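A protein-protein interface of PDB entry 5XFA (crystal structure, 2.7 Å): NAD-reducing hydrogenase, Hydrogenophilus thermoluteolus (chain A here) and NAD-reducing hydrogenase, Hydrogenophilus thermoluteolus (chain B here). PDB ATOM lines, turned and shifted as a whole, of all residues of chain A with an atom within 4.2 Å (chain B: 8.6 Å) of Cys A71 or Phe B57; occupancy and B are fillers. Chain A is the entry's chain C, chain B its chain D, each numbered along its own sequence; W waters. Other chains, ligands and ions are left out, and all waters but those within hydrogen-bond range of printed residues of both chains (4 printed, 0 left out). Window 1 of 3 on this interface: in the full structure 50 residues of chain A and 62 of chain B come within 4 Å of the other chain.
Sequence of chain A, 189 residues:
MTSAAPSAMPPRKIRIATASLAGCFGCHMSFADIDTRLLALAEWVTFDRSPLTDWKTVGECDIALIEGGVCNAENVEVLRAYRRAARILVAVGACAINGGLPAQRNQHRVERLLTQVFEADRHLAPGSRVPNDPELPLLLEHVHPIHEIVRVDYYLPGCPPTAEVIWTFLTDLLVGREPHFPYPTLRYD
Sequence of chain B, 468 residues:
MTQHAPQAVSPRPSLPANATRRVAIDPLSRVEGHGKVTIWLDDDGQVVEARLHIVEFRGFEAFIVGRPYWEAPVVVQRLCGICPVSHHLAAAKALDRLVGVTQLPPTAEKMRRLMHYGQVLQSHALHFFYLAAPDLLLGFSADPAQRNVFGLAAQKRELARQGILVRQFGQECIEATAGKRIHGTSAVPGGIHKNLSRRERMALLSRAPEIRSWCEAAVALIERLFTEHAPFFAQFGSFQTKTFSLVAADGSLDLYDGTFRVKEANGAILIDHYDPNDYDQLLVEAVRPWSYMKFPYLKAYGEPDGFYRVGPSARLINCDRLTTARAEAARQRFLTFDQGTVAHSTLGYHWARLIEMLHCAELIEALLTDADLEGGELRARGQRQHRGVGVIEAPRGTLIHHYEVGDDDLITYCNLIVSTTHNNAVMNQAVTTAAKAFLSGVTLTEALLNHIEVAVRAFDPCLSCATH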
ATOM      1  N   ALA A  22      22.872 -29.591  17.924  1.00  0.00           N
ATOM      2  CA  ALA A  22      23.527 -28.581  17.104  1.00  0.00           C
ATOM      3  C   ALA A  22      24.219 -29.215  15.878  1.00  0.00           C
ATOM      4  O   ALA A  22      25.403 -28.917  15.578  1.00  0.00           O
ATOM      5  CB  ALA A  22      24.520 -27.792  17.933  1.00  0.00           C
ATOM      6  N   GLY A  69      26.290 -31.181  18.426  1.00  0.00           N
ATOM      7  CA  GLY A  69      26.731 -30.779  19.774  1.00  0.00           C
ATOM      8  C   GLY A  69      25.555 -30.278  20.593  1.00  0.00           C
ATOM      9  O   GLY A  69      24.418 -30.400  20.156  1.00  0.00           O
ATOM     10  N   VAL A  70      25.800 -29.756  21.794  1.00  0.00           N
ATOM     11  CA  VAL A  70      24.738 -29.034  22.525  1.00  0.00           C
ATOM     12  C   VAL A  70      25.128 -27.578  22.532  1.00  0.00           C
ATOM     13  O   VAL A  70      26.233 -27.213  22.966  1.00  0.00           O
ATOM     14  CB  VAL A  70      24.432 -29.569  23.943  1.00  0.00           C
ATOM     15  CG1 VAL A  70      24.112 -31.050  23.870  1.00  0.00           C
ATOM     16  CG2 VAL A  70      25.579 -29.330  24.903  1.00  0.00           C
ATOM     17  N   CYS A  71      24.218 -26.768  21.991  1.00  0.00           N
ATOM     18  CA  CYS A  71      24.449 -25.352  21.683  1.00  0.00           C
ATOM     19  C   CYS A  71      23.477 -24.435  22.429  1.00  0.00           C
ATOM     20  O   CYS A  71      23.786 -23.275  22.671  1.00  0.00           O
ATOM     21  CB  CYS A  71      24.304 -25.145  20.162  1.00  0.00           C
ATOM     22  SG  CYS A  71      24.688 -23.492  19.543  1.00  0.00           S
ATOM     23  N   ASN A  72      22.295 -24.952  22.749  1.00  0.00           N
ATOM     24  CA  ASN A  72      21.243 -24.163  23.346  1.00  0.00           C
ATOM     25  C   ASN A  72      20.423 -25.004  24.317  1.00  0.00           C
ATOM     26  O   ASN A  72      20.601 -26.218  24.418  1.00  0.00           O
ATOM     27  CB  ASN A  72      20.360 -23.548  22.258  1.00  0.00           C
ATOM     28  CG  ASN A  72      19.537 -24.574  21.515  1.00  0.00           C
ATOM     29  OD1 ASN A  72      18.740 -25.305  22.114  1.00  0.00           O
ATOM     30  ND2 ASN A  72      19.690 -24.611  20.193  1.00  0.00           N
ATOM     31  N   ASN A  75      18.441 -28.153  23.244  1.00  0.00           N
ATOM     32  CA  ASN A  75      19.285 -29.317  22.968  1.00  0.00           C
ATOM     33  C   ASN A  75      19.457 -30.142  24.226  1.00  0.00           C
ATOM     34  O   ASN A  75      19.471 -31.367  24.167  1.00  0.00           O
ATOM     35  CB  ASN A  75      20.681 -28.936  22.488  1.00  0.00           C
ATOM     36  CG  ASN A  75      20.700 -28.295  21.135  1.00  0.00           C
ATOM     37  OD1 ASN A  75      21.659 -27.577  20.804  1.00  0.00           O
ATOM     38  ND2 ASN A  75      19.656 -28.537  20.335  1.00  0.00           N
ATOM     39  N   ARG A 105      33.026 -21.505  17.837  1.00  0.00           N
ATOM     40  CA  ARG A 105      32.405 -20.313  18.448  1.00  0.00           C
ATOM     41  C   ARG A 105      32.840 -20.095  19.906  1.00  0.00           C
ATOM     42  O   ARG A 105      32.710 -18.988  20.428  1.00  0.00           O
ATOM     43  CB  ARG A 105      30.857 -20.318  18.294  1.00  0.00           C
ATOM     44  CG  ARG A 105      30.038 -20.933  19.418  1.00  0.00           C
ATOM     45  CD  ARG A 105      28.541 -20.649  19.241  1.00  0.00           C
ATOM     46  NE  ARG A 105      27.686 -21.451  20.135  1.00  0.00           N
ATOM     47  CZ  ARG A 105      27.436 -21.161  21.424  1.00  0.00           C
ATOM     48  NH1 ARG A 105      27.937 -20.077  22.003  1.00  0.00           N
ATOM     49  NH2 ARG A 105      26.663 -21.961  22.149  1.00  0.00           N
ATOM     50  N   LEU A 114      25.860 -12.883  18.651  1.00  0.00           N
ATOM     51  CA  LEU A 114      24.455 -12.627  18.344  1.00  0.00           C
ATOM     52  C   LEU A 114      24.262 -11.182  17.940  1.00  0.00           C
ATOM     53  O   LEU A 114      23.446 -10.845  17.067  1.00  0.00           O
ATOM     54  CB  LEU A 114      23.595 -12.941  19.563  1.00  0.00           C
ATOM     55  CG  LEU A 114      23.393 -14.425  19.870  1.00  0.00           C
ATOM     56  CD1 LEU A 114      22.977 -14.617  21.321  1.00  0.00           C
ATOM     57  CD2 LEU A 114      22.352 -15.036  18.955  1.00  0.00           C
ATOM     58  N   VAL A 117      25.534 -10.571  14.444  1.00  0.00           N
ATOM     59  CA  VAL A 117      24.691 -11.098  13.389  1.00  0.00           C
ATOM     60  C   VAL A 117      23.359 -10.386  13.297  1.00  0.00           C
ATOM     61  O   VAL A 117      22.895 -10.101  12.198  1.00  0.00           O
ATOM     62  CB  VAL A 117      24.443 -12.591  13.593  1.00  0.00           C
ATOM     63  CG1 VAL A 117      23.589 -13.150  12.470  1.00  0.00           C
ATOM     64  CG2 VAL A 117      25.776 -13.317  13.672  1.00  0.00           C
ATOM     65  N   PHE A 118      22.746 -10.099  14.444  1.00  0.00           N
ATOM     66  CA  PHE A 118      21.371  -9.585  14.475  1.00  0.00           C
ATOM     67  C   PHE A 118      21.230  -8.074  14.754  1.00  0.00           C
ATOM     68  O   PHE A 118      20.122  -7.525  14.614  1.00  0.00           O
ATOM     69  CB  PHE A 118      20.557 -10.364  15.496  1.00  0.00           C
ATOM     70  CG  PHE A 118      20.336 -11.788  15.118  1.00  0.00           C
ATOM     71  CD1 PHE A 118      19.353 -12.125  14.217  1.00  0.00           C
ATOM     72  CD2 PHE A 118      21.088 -12.796  15.677  1.00  0.00           C
ATOM     73  CE1 PHE A 118      19.130 -13.443  13.859  1.00  0.00           C
ATOM     74  CE2 PHE A 118      20.866 -14.130  15.329  1.00  0.00           C
ATOM     75  CZ  PHE A 118      19.894 -14.450  14.410  1.00  0.00           C
ATOM     76  N   LEU A 139      21.010 -19.647  23.672  1.00  0.00           N
ATOM     77  CA  LEU A 139      22.327 -20.258  23.493  1.00  0.00           C
ATOM     78  C   LEU A 139      23.109 -20.374  24.806  1.00  0.00           C
ATOM     79  O   LEU A 139      23.056 -19.483  25.653  1.00  0.00           O
ATOM     80  CB  LEU A 139      23.160 -19.440  22.491  1.00  0.00           C
ATOM     81  CG  LEU A 139      22.995 -19.798  21.007  1.00  0.00           C
ATOM     82  CD1 LEU A 139      21.540 -19.811  20.596  1.00  0.00           C
ATOM     83  CD2 LEU A 139      23.793 -18.840  20.134  1.00  0.00           C
ATOM     84  N   LEU A 140      23.848 -21.471  24.953  1.00  0.00           N
ATOM     85  CA  LEU A 140      24.777 -21.660  26.072  1.00  0.00           C
ATOM     86  C   LEU A 140      26.026 -20.838  25.844  1.00  0.00           C
ATOM     87  O   LEU A 140      26.292 -20.377  24.742  1.00  0.00           O
ATOM     88  CB  LEU A 140      25.158 -23.139  26.233  1.00  0.00           C
ATOM     89  CG  LEU A 140      24.151 -24.093  26.898  1.00  0.00           C
ATOM     90  CD1 LEU A 140      22.738 -23.821  26.443  1.00  0.00           C
ATOM     91  CD2 LEU A 140      24.486 -25.537  26.571  1.00  0.00           C
ATOM     92  N   HIS B  34      15.637 -27.415  12.989  1.00  0.00           N
ATOM     93  CA  HIS B  34      14.772 -27.271  14.147  1.00  0.00           C
ATOM     94  C   HIS B  34      13.862 -26.098  13.946  1.00  0.00           C
ATOM     95  O   HIS B  34      14.285 -24.937  14.030  1.00  0.00           O
ATOM     96  CB  HIS B  34      15.570 -27.063  15.425  1.00  0.00           C
ATOM     97  CG  HIS B  34      16.655 -28.061  15.623  1.00  0.00           C
ATOM     98  ND1 HIS B  34      16.567 -29.348  15.151  1.00  0.00           N
ATOM     99  CD2 HIS B  34      17.858 -27.962  16.232  1.00  0.00           C
ATOM    100  CE1 HIS B  34      17.675 -29.998  15.448  1.00  0.00           C
ATOM    101  NE2 HIS B  34      18.470 -29.185  16.116  1.00  0.00           N
ATOM    102  N   ILE B  54      11.982 -20.356  13.772  1.00  0.00           N
ATOM    103  CA  ILE B  54      13.172 -21.137  13.485  1.00  0.00           C
ATOM    104  C   ILE B  54      14.053 -20.989  14.683  1.00  0.00           C
ATOM    105  O   ILE B  54      14.523 -19.903  15.019  1.00  0.00           O
ATOM    106  CB  ILE B  54      13.911 -20.744  12.185  1.00  0.00           C
ATOM    107  CG1 ILE B  54      12.928 -20.670  11.029  1.00  0.00           C
ATOM    108  CG2 ILE B  54      14.978 -21.791  11.868  1.00  0.00           C
ATOM    109  CD1 ILE B  54      12.020 -21.888  10.932  1.00  0.00           C
ATOM    110  N   VAL B  55      14.306 -22.126  15.285  1.00  0.00           N
ATOM    111  CA  VAL B  55      14.571 -22.199  16.699  1.00  0.00           C
ATOM    112  C   VAL B  55      16.072 -22.558  17.030  1.00  0.00           C
ATOM    113  O   VAL B  55      16.424 -22.764  18.186  1.00  0.00           O
ATOM    114  CB  VAL B  55      13.502 -23.178  17.280  1.00  0.00           C
ATOM    115  CG1 VAL B  55      13.984 -24.628  17.254  1.00  0.00           C
ATOM    116  CG2 VAL B  55      13.018 -22.759  18.665  1.00  0.00           C
ATOM    117  N   GLU B  56      16.931 -22.600  16.007  1.00  0.00           N
ATOM    118  CA  GLU B  56      18.352 -22.929  16.159  1.00  0.00           C
ATOM    119  C   GLU B  56      19.258 -21.871  15.524  1.00  0.00           C
ATOM    120  O   GLU B  56      18.872 -21.191  14.564  1.00  0.00           O
ATOM    121  CB  GLU B  56      18.668 -24.291  15.524  1.00  0.00           C
ATOM    122  CG  GLU B  56      18.510 -24.366  13.995  1.00  0.00           C
ATOM    123  CD  GLU B  56      19.334 -25.491  13.357  1.00  0.00           C
ATOM    124  OE1 GLU B  56      20.579 -25.505  13.509  1.00  0.00           O
ATOM    125  OE2 GLU B  56      18.750 -26.365  12.690  1.00  0.00           O
ATOM    126  N   PHE B  57      20.471 -21.754  16.052  1.00  0.00           N
ATOM    127  CA  PHE B  57      21.441 -20.796  15.546  1.00  0.00           C
ATOM    128  C   PHE B  57      22.840 -21.121  16.042  1.00  0.00           C
ATOM    129  O   PHE B  57      23.038 -21.349  17.246  1.00  0.00           O
ATOM    130  CB  PHE B  57      21.069 -19.405  16.008  1.00  0.00           C
ATOM    131  CG  PHE B  57      22.109 -18.372  15.710  1.00  0.00           C
ATOM    132  CD1 PHE B  57      22.253 -17.862  14.433  1.00  0.00           C
ATOM    133  CD2 PHE B  57      22.926 -17.889  16.713  1.00  0.00           C
ATOM    134  CE1 PHE B  57      23.211 -16.901  14.164  1.00  0.00           C
ATOM    135  CE2 PHE B  57      23.876 -16.923  16.452  1.00  0.00           C
ATOM    136  CZ  PHE B  57      24.007 -16.417  15.177  1.00  0.00           C
ATOM    137  N   ARG B  58      23.807 -21.125  15.118  1.00  0.00           N
ATOM    138  CA  ARG B  58      25.185 -21.501  15.420  1.00  0.00           C
ATOM    139  C   ARG B  58      26.196 -20.377  15.217  1.00  0.00           C
ATOM    140  O   ARG B  58      27.256 -20.366  15.846  1.00  0.00           O
ATOM    141  CB  ARG B  58      25.564 -22.720  14.595  1.00  0.00           C
ATOM    142  CG  ARG B  58      24.827 -23.978  15.055  1.00  0.00           C
ATOM    143  CD  ARG B  58      24.882 -25.090  14.018  1.00  0.00           C
ATOM    144  NE  ARG B  58      24.235 -24.670  12.771  1.00  0.00           N
ATOM    145  CZ  ARG B  58      24.475 -25.182  11.560  1.00  0.00           C
ATOM    146  NH1 ARG B  58      25.358 -26.171  11.391  1.00  0.00           N
ATOM    147  NH2 ARG B  58      23.821 -24.694  10.507  1.00  0.00           N
ATOM    148  N   GLY B  59      25.894 -19.449  14.318  1.00  0.00           N
ATOM    149  CA  GLY B  59      26.656 -18.212  14.182  1.00  0.00           C
ATOM    150  C   GLY B  59      27.867 -18.306  13.294  1.00  0.00           C
ATOM    151  O   GLY B  59      28.885 -17.665  13.590  1.00  0.00           O
ATOM    152  N   PHE B  60      27.750 -19.061  12.193  1.00  0.00           N
ATOM    153  CA  PHE B  60      28.873 -19.244  11.239  1.00  0.00           C
ATOM    154  C   PHE B  60      29.465 -17.934  10.692  1.00  0.00           C
ATOM    155  O   PHE B  60      30.649 -17.860  10.434  1.00  0.00           O
ATOM    156  CB  PHE B  60      28.470 -20.111  10.043  1.00  0.00           C
ATOM    157  CG  PHE B  60      28.547 -21.595  10.293  1.00  0.00           C
ATOM    158  CD1 PHE B  60      29.575 -22.346   9.759  1.00  0.00           C
ATOM    159  CD2 PHE B  60      27.573 -22.250  11.038  1.00  0.00           C
ATOM    160  CE1 PHE B  60      29.654 -23.715   9.982  1.00  0.00           C
ATOM    161  CE2 PHE B  60      27.632 -23.621  11.242  1.00  0.00           C
ATOM    162  CZ  PHE B  60      28.679 -24.353  10.716  1.00  0.00           C
ATOM    163  N   GLU B  61      28.646 -16.906  10.549  1.00  0.00           N
ATOM    164  CA  GLU B  61      29.081 -15.634   9.971  1.00  0.00           C
ATOM    165  C   GLU B  61      30.065 -14.899  10.899  1.00  0.00           C
ATOM    166  O   GLU B  61      30.865 -14.066  10.456  1.00  0.00           O
ATOM    167  CB  GLU B  61      27.849 -14.754   9.700  1.00  0.00           C
ATOM    168  CG  GLU B  61      26.833 -15.416   8.746  1.00  0.00           C
ATOM    169  CD  GLU B  61      25.500 -14.711   8.647  1.00  0.00           C
ATOM    170  OE1 GLU B  61      25.003 -14.218   9.675  1.00  0.00           O
ATOM    171  OE2 GLU B  61      24.949 -14.697   7.537  1.00  0.00           O
ATOM    172  N   ALA B  62      29.983 -15.210  12.182  1.00  0.00           N
ATOM    173  CA  ALA B  62      30.728 -14.499  13.179  1.00  0.00           C
ATOM    174  C   ALA B  62      31.955 -15.283  13.654  1.00  0.00           C
ATOM    175  O   ALA B  62      32.996 -14.673  13.925  1.00  0.00           O
ATOM    176  CB  ALA B  62      29.827 -14.179  14.347  1.00  0.00           C
ATOM    177  N   PHE B  63      31.837 -16.611  13.734  1.00  0.00           N
ATOM    178  CA  PHE B  63      32.957 -17.454  14.175  1.00  0.00           C
ATOM    179  C   PHE B  63      33.952 -17.863  13.080  1.00  0.00           C
ATOM    180  O   PHE B  63      35.127 -18.130  13.390  1.00  0.00           O
ATOM    181  CB  PHE B  63      32.489 -18.650  15.043  1.00  0.00           C
ATOM    182  CG  PHE B  63      31.930 -19.819  14.283  1.00  0.00           C
ATOM    183  CD1 PHE B  63      32.723 -20.552  13.391  1.00  0.00           C
ATOM    184  CD2 PHE B  63      30.621 -20.246  14.525  1.00  0.00           C
ATOM    185  CE1 PHE B  63      32.202 -21.655  12.714  1.00  0.00           C
ATOM    186  CE2 PHE B  63      30.090 -21.349  13.855  1.00  0.00           C
ATOM    187  CZ  PHE B  63      30.880 -22.055  12.943  1.00  0.00           C
ATOM    188  N   SER B 291      12.085 -15.476  15.653  1.00  0.00           N
ATOM    189  CA  SER B 291      12.768 -16.462  14.819  1.00  0.00           C
ATOM    190  C   SER B 291      14.236 -16.095  14.713  1.00  0.00           C
ATOM    191  O   SER B 291      14.572 -14.913  14.797  1.00  0.00           O
ATOM    192  CB  SER B 291      12.150 -16.522  13.435  1.00  0.00           C
ATOM    193  OG  SER B 291      12.602 -17.648  12.711  1.00  0.00           O
ATOM    194  N   TYR B 292      15.114 -17.095  14.575  1.00  0.00           N
ATOM    195  CA  TYR B 292      16.536 -16.833  14.294  1.00  0.00           C
ATOM    196  C   TYR B 292      16.778 -16.687  12.778  1.00  0.00           C
ATOM    197  O   TYR B 292      17.850 -16.260  12.353  1.00  0.00           O
ATOM    198  CB  TYR B 292      17.419 -17.934  14.844  1.00  0.00           C
ATOM    199  CG  TYR B 292      17.577 -17.900  16.332  1.00  0.00           C
ATOM    200  CD1 TYR B 292      18.263 -16.863  16.951  1.00  0.00           C
ATOM    201  CD2 TYR B 292      17.075 -18.922  17.125  1.00  0.00           C
ATOM    202  CE1 TYR B 292      18.429 -16.837  18.326  1.00  0.00           C
ATOM    203  CE2 TYR B 292      17.229 -18.903  18.500  1.00  0.00           C
ATOM    204  CZ  TYR B 292      17.904 -17.864  19.101  1.00  0.00           C
ATOM    205  OH  TYR B 292      18.051 -17.856  20.471  1.00  0.00           O
ATOM    206  N   MET B 293      15.765 -17.032  11.983  1.00  0.00           N
ATOM    207  CA  MET B 293      15.787 -16.845  10.529  1.00  0.00           C
ATOM    208  C   MET B 293      15.425 -15.404  10.227  1.00  0.00           C
ATOM    209  O   MET B 293      14.426 -14.915  10.723  1.00  0.00           O
ATOM    210  CB  MET B 293      14.759 -17.780   9.874  1.00  0.00           C
ATOM    211  CG  MET B 293      14.893 -17.985   8.375  1.00  0.00           C
ATOM    212  SD  MET B 293      13.963 -19.463   7.899  1.00  0.00           S
ATOM    213  CE  MET B 293      13.079 -18.894   6.473  1.00  0.00           C
ATOM    214  N   LYS B 294      16.243 -14.735   9.420  1.00  0.00           N
ATOM    215  CA  LYS B 294      16.048 -13.332   9.117  1.00  0.00           C
ATOM    216  C   LYS B 294      14.989 -13.176   8.035  1.00  0.00           C
ATOM    217  O   LYS B 294      14.438 -14.158   7.564  1.00  0.00           O
ATOM    218  CB  LYS B 294      17.359 -12.689   8.693  1.00  0.00           C
ATOM    219  CG  LYS B 294      18.372 -12.566   9.811  1.00  0.00           C
ATOM    220  CD  LYS B 294      19.613 -11.865   9.298  1.00  0.00           C
ATOM    221  CE  LYS B 294      20.743 -11.886  10.326  1.00  0.00           C
ATOM    222  NZ  LYS B 294      21.942 -11.172   9.824  1.00  0.00           N
ATOM    223  N   LEU B 463      16.466 -25.505   7.589  1.00  0.00           N
ATOM    224  CA  LEU B 463      16.423 -24.514   8.674  1.00  0.00           C
ATOM    225  C   LEU B 463      17.820 -24.264   9.257  1.00  0.00           C
ATOM    226  O   LEU B 463      18.121 -23.141   9.685  1.00  0.00           O
ATOM    227  CB  LEU B 463      15.420 -24.949   9.734  1.00  0.00           C
ATOM    228  CG  LEU B 463      14.021 -25.173   9.135  1.00  0.00           C
ATOM    229  CD1 LEU B 463      13.047 -25.799  10.122  1.00  0.00           C
ATOM    230  CD2 LEU B 463      13.453 -23.868   8.596  1.00  0.00           C
ATOM    231  N   SER B 464      18.679 -25.290   9.238  1.00  0.00           N
ATOM    232  CA  SER B 464      20.096 -25.121   9.551  1.00  0.00           C
ATOM    233  C   SER B 464      20.720 -24.149   8.569  1.00  0.00           C
ATOM    234  O   SER B 464      21.461 -23.260   8.932  1.00  0.00           O
ATOM    235  CB  SER B 464      20.838 -26.459   9.459  1.00  0.00           C
ATOM    236  OG  SER B 464      20.195 -27.468  10.223  1.00  0.00           O
ATOM    237  N   ALA B 466      19.086 -21.983   6.869  1.00  0.00           N
ATOM    238  CA  ALA B 466      18.370 -20.711   6.973  1.00  0.00           C
ATOM    239  C   ALA B 466      18.904 -19.777   8.041  1.00  0.00           C
ATOM    240  O   ALA B 466      18.831 -18.549   7.893  1.00  0.00           O
ATOM    241  CB  ALA B 466      16.903 -20.983   7.238  1.00  0.00           C
ATOM    242  N   THR B 467      19.446 -20.385   9.092  1.00  0.00           N
ATOM    243  CA  THR B 467      19.858 -19.689  10.292  1.00  0.00           C
ATOM    244  C   THR B 467      21.370 -19.451  10.385  1.00  0.00           C
ATOM    245  O   THR B 467      21.843 -18.333  10.713  1.00  0.00           O
ATOM    246  CB  THR B 467      19.450 -20.526  11.510  1.00  0.00           C
ATOM    247  OG1 THR B 467      19.834 -21.903  11.303  1.00  0.00           O
ATOM    248  CG2 THR B 467      17.955 -20.430  11.706  1.00  0.00           C
ATOM    249  N   HIS B 468      22.091 -20.538  10.109  1.00  0.00           N
ATOM    250  CA  HIS B 468      23.548 -20.627  10.120  1.00  0.00           C
ATOM    251  C   HIS B 468      24.106 -19.872  11.246  1.00  0.00           C
ATOM    252  O   HIS B 468      25.003 -19.038  11.062  1.00  0.00           O
ATOM    253  CB  HIS B 468      24.144 -20.164   8.799  1.00  0.00           C
ATOM    254  CG  HIS B 468      23.524 -18.929   8.254  1.00  0.00           C
ATOM    255  ND1 HIS B 468      22.429 -18.956   7.427  1.00  0.00           N
ATOM    256  CD2 HIS B 468      23.848 -17.623   8.410  1.00  0.00           C
ATOM    257  CE1 HIS B 468      22.100 -17.719   7.096  1.00  0.00           C
ATOM    258  NE2 HIS B 468      22.953 -16.892   7.676  1.00  0.00           N
ATOM    259  OXT HIS B 468      23.604 -20.142  12.333  1.00  0.00           O
HETATM  260  O   HOH W   1      28.258 -22.507  16.996  1.00  0.00           O
HETATM  261  O   HOH W   2      21.806 -23.224  18.890  1.00  0.00           O
HETATM  262  O   HOH W   3      20.290 -26.944  17.776  1.00  0.00           O
HETATM  263  O   HOH W   4      26.547 -28.192  12.907  1.00  0.00           O
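OD1 of Asn A75 is in hydrogen-bond range of N of Cys A71 (2.9 Å).
NH2 of Arg B58 lies within hydrogen-bond range of O of Ser B464.
The chain-end carboxylate (OXT) of His B468 lies within hydrogen-bond range of the backbone NH (N) of Arg B58 (3.0 Å).
The guanidinium group (NH2) of Arg A105 lies within hydrogen-bond range of the backbone carbonyl oxygen (O) of Leu A140 (3.1 Å).
OE1 of Glu B56 is in salt-bridge range of NE of Arg B58.
The backbone NH (N) of Tyr B292 lies within hydrogen-bond range of the backbone carbonyl oxygen (O) of Ile B54.
Hydrophobic or aromatic side chains of chain B that line the printed part of chain A: Phe B57, Phe B63 and Tyr B292.
Printed residues of chain A that touch a printed residue of chain B: Cys A71, Arg A105, Leu A114, Val A117, Phe A118 and Leu A139.
Hydrophobic or aromatic side chains of chain A within 4 Å of the printed part of chain B: Leu A114, Val A117, Phe A118 and Leu A139.
Along chain A the printed residues that touch a printed residue of chain B span positions 71 to 139.
Among the printed residues, 10 pairs touch across the chains.
Among the printed residues, merely in contact across the chains: Arg A105 with Arg B58 (3.6 Å), Arg A105 with Phe B63 (3.8 Å), Leu A114 with Phe B57 (3.5 Å), Val A117 with Phe B57 (3.9 Å), Val A117 with Glu B61 (3.3 Å), Phe A118 with Phe B57 (3.8 Å), Phe A118 with Tyr B292 (3.4 Å) and Leu A139 with Phe B57 (3.7 Å).
Cys A71 touches just one residue of chain B: Phe B57 (3.5 Å).
Phe B57 touches just these residues of chain A: Cys A71 (3.5 Å), Leu A114 (3.5 Å), Val A117 (3.9 Å), Phe A118 (3.8 Å) and Leu A139 (3.7 Å).
Printed residues of chain A within 4 Å of Arg B58: Arg A105.
Of the printed residues of chain B, Leu A114 touches Phe B57 (3.5 Å).
Of the printed residues of chain B, Leu A139 touches Phe B57 (3.7 Å).
The nearest printed residue of chain A that does not touch Phe B57 is Asn A72 (5.1 Å).
The nearest printed residue of chain B that does not touch Val A117 is Ala B62 (4.2 Å).
The backbone carbonyl oxygen (O) of Val A117 lies within hydrogen-bond range of the side-chain amino group (NZ) of Lys B294 (2.8 Å).
The backbone carbonyl oxygen (O) of Phe B57 sits at hydrogen-bond distance from the side-chain sulfur (SG) of Cys A71, at 3.5 Å.
Water W1 lies within hydrogen-bond range of O of Arg B58 (2.6 Å) and NE of Arg A105 (3.4 Å).
Water W2 lies within hydrogen-bond range of the backbone carbonyl oxygen of Phe B57 (2.8 Å), the side-chain amide nitrogen of Asn A72 (2.8 Å) and the side-chain sulfur of Cys A71 (3.0 Å).
Water W4 bridges the guanidinium group (NH1) of Arg B58 and the backbone carbonyl oxygen (O) of Ala A22.
Water W3 lies within hydrogen-bond range of ND2 of Asn A75 (3.1 Å), NE2 of His B34 (3.3 Å) and ND2 of Asn A72 (3.4 Å).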
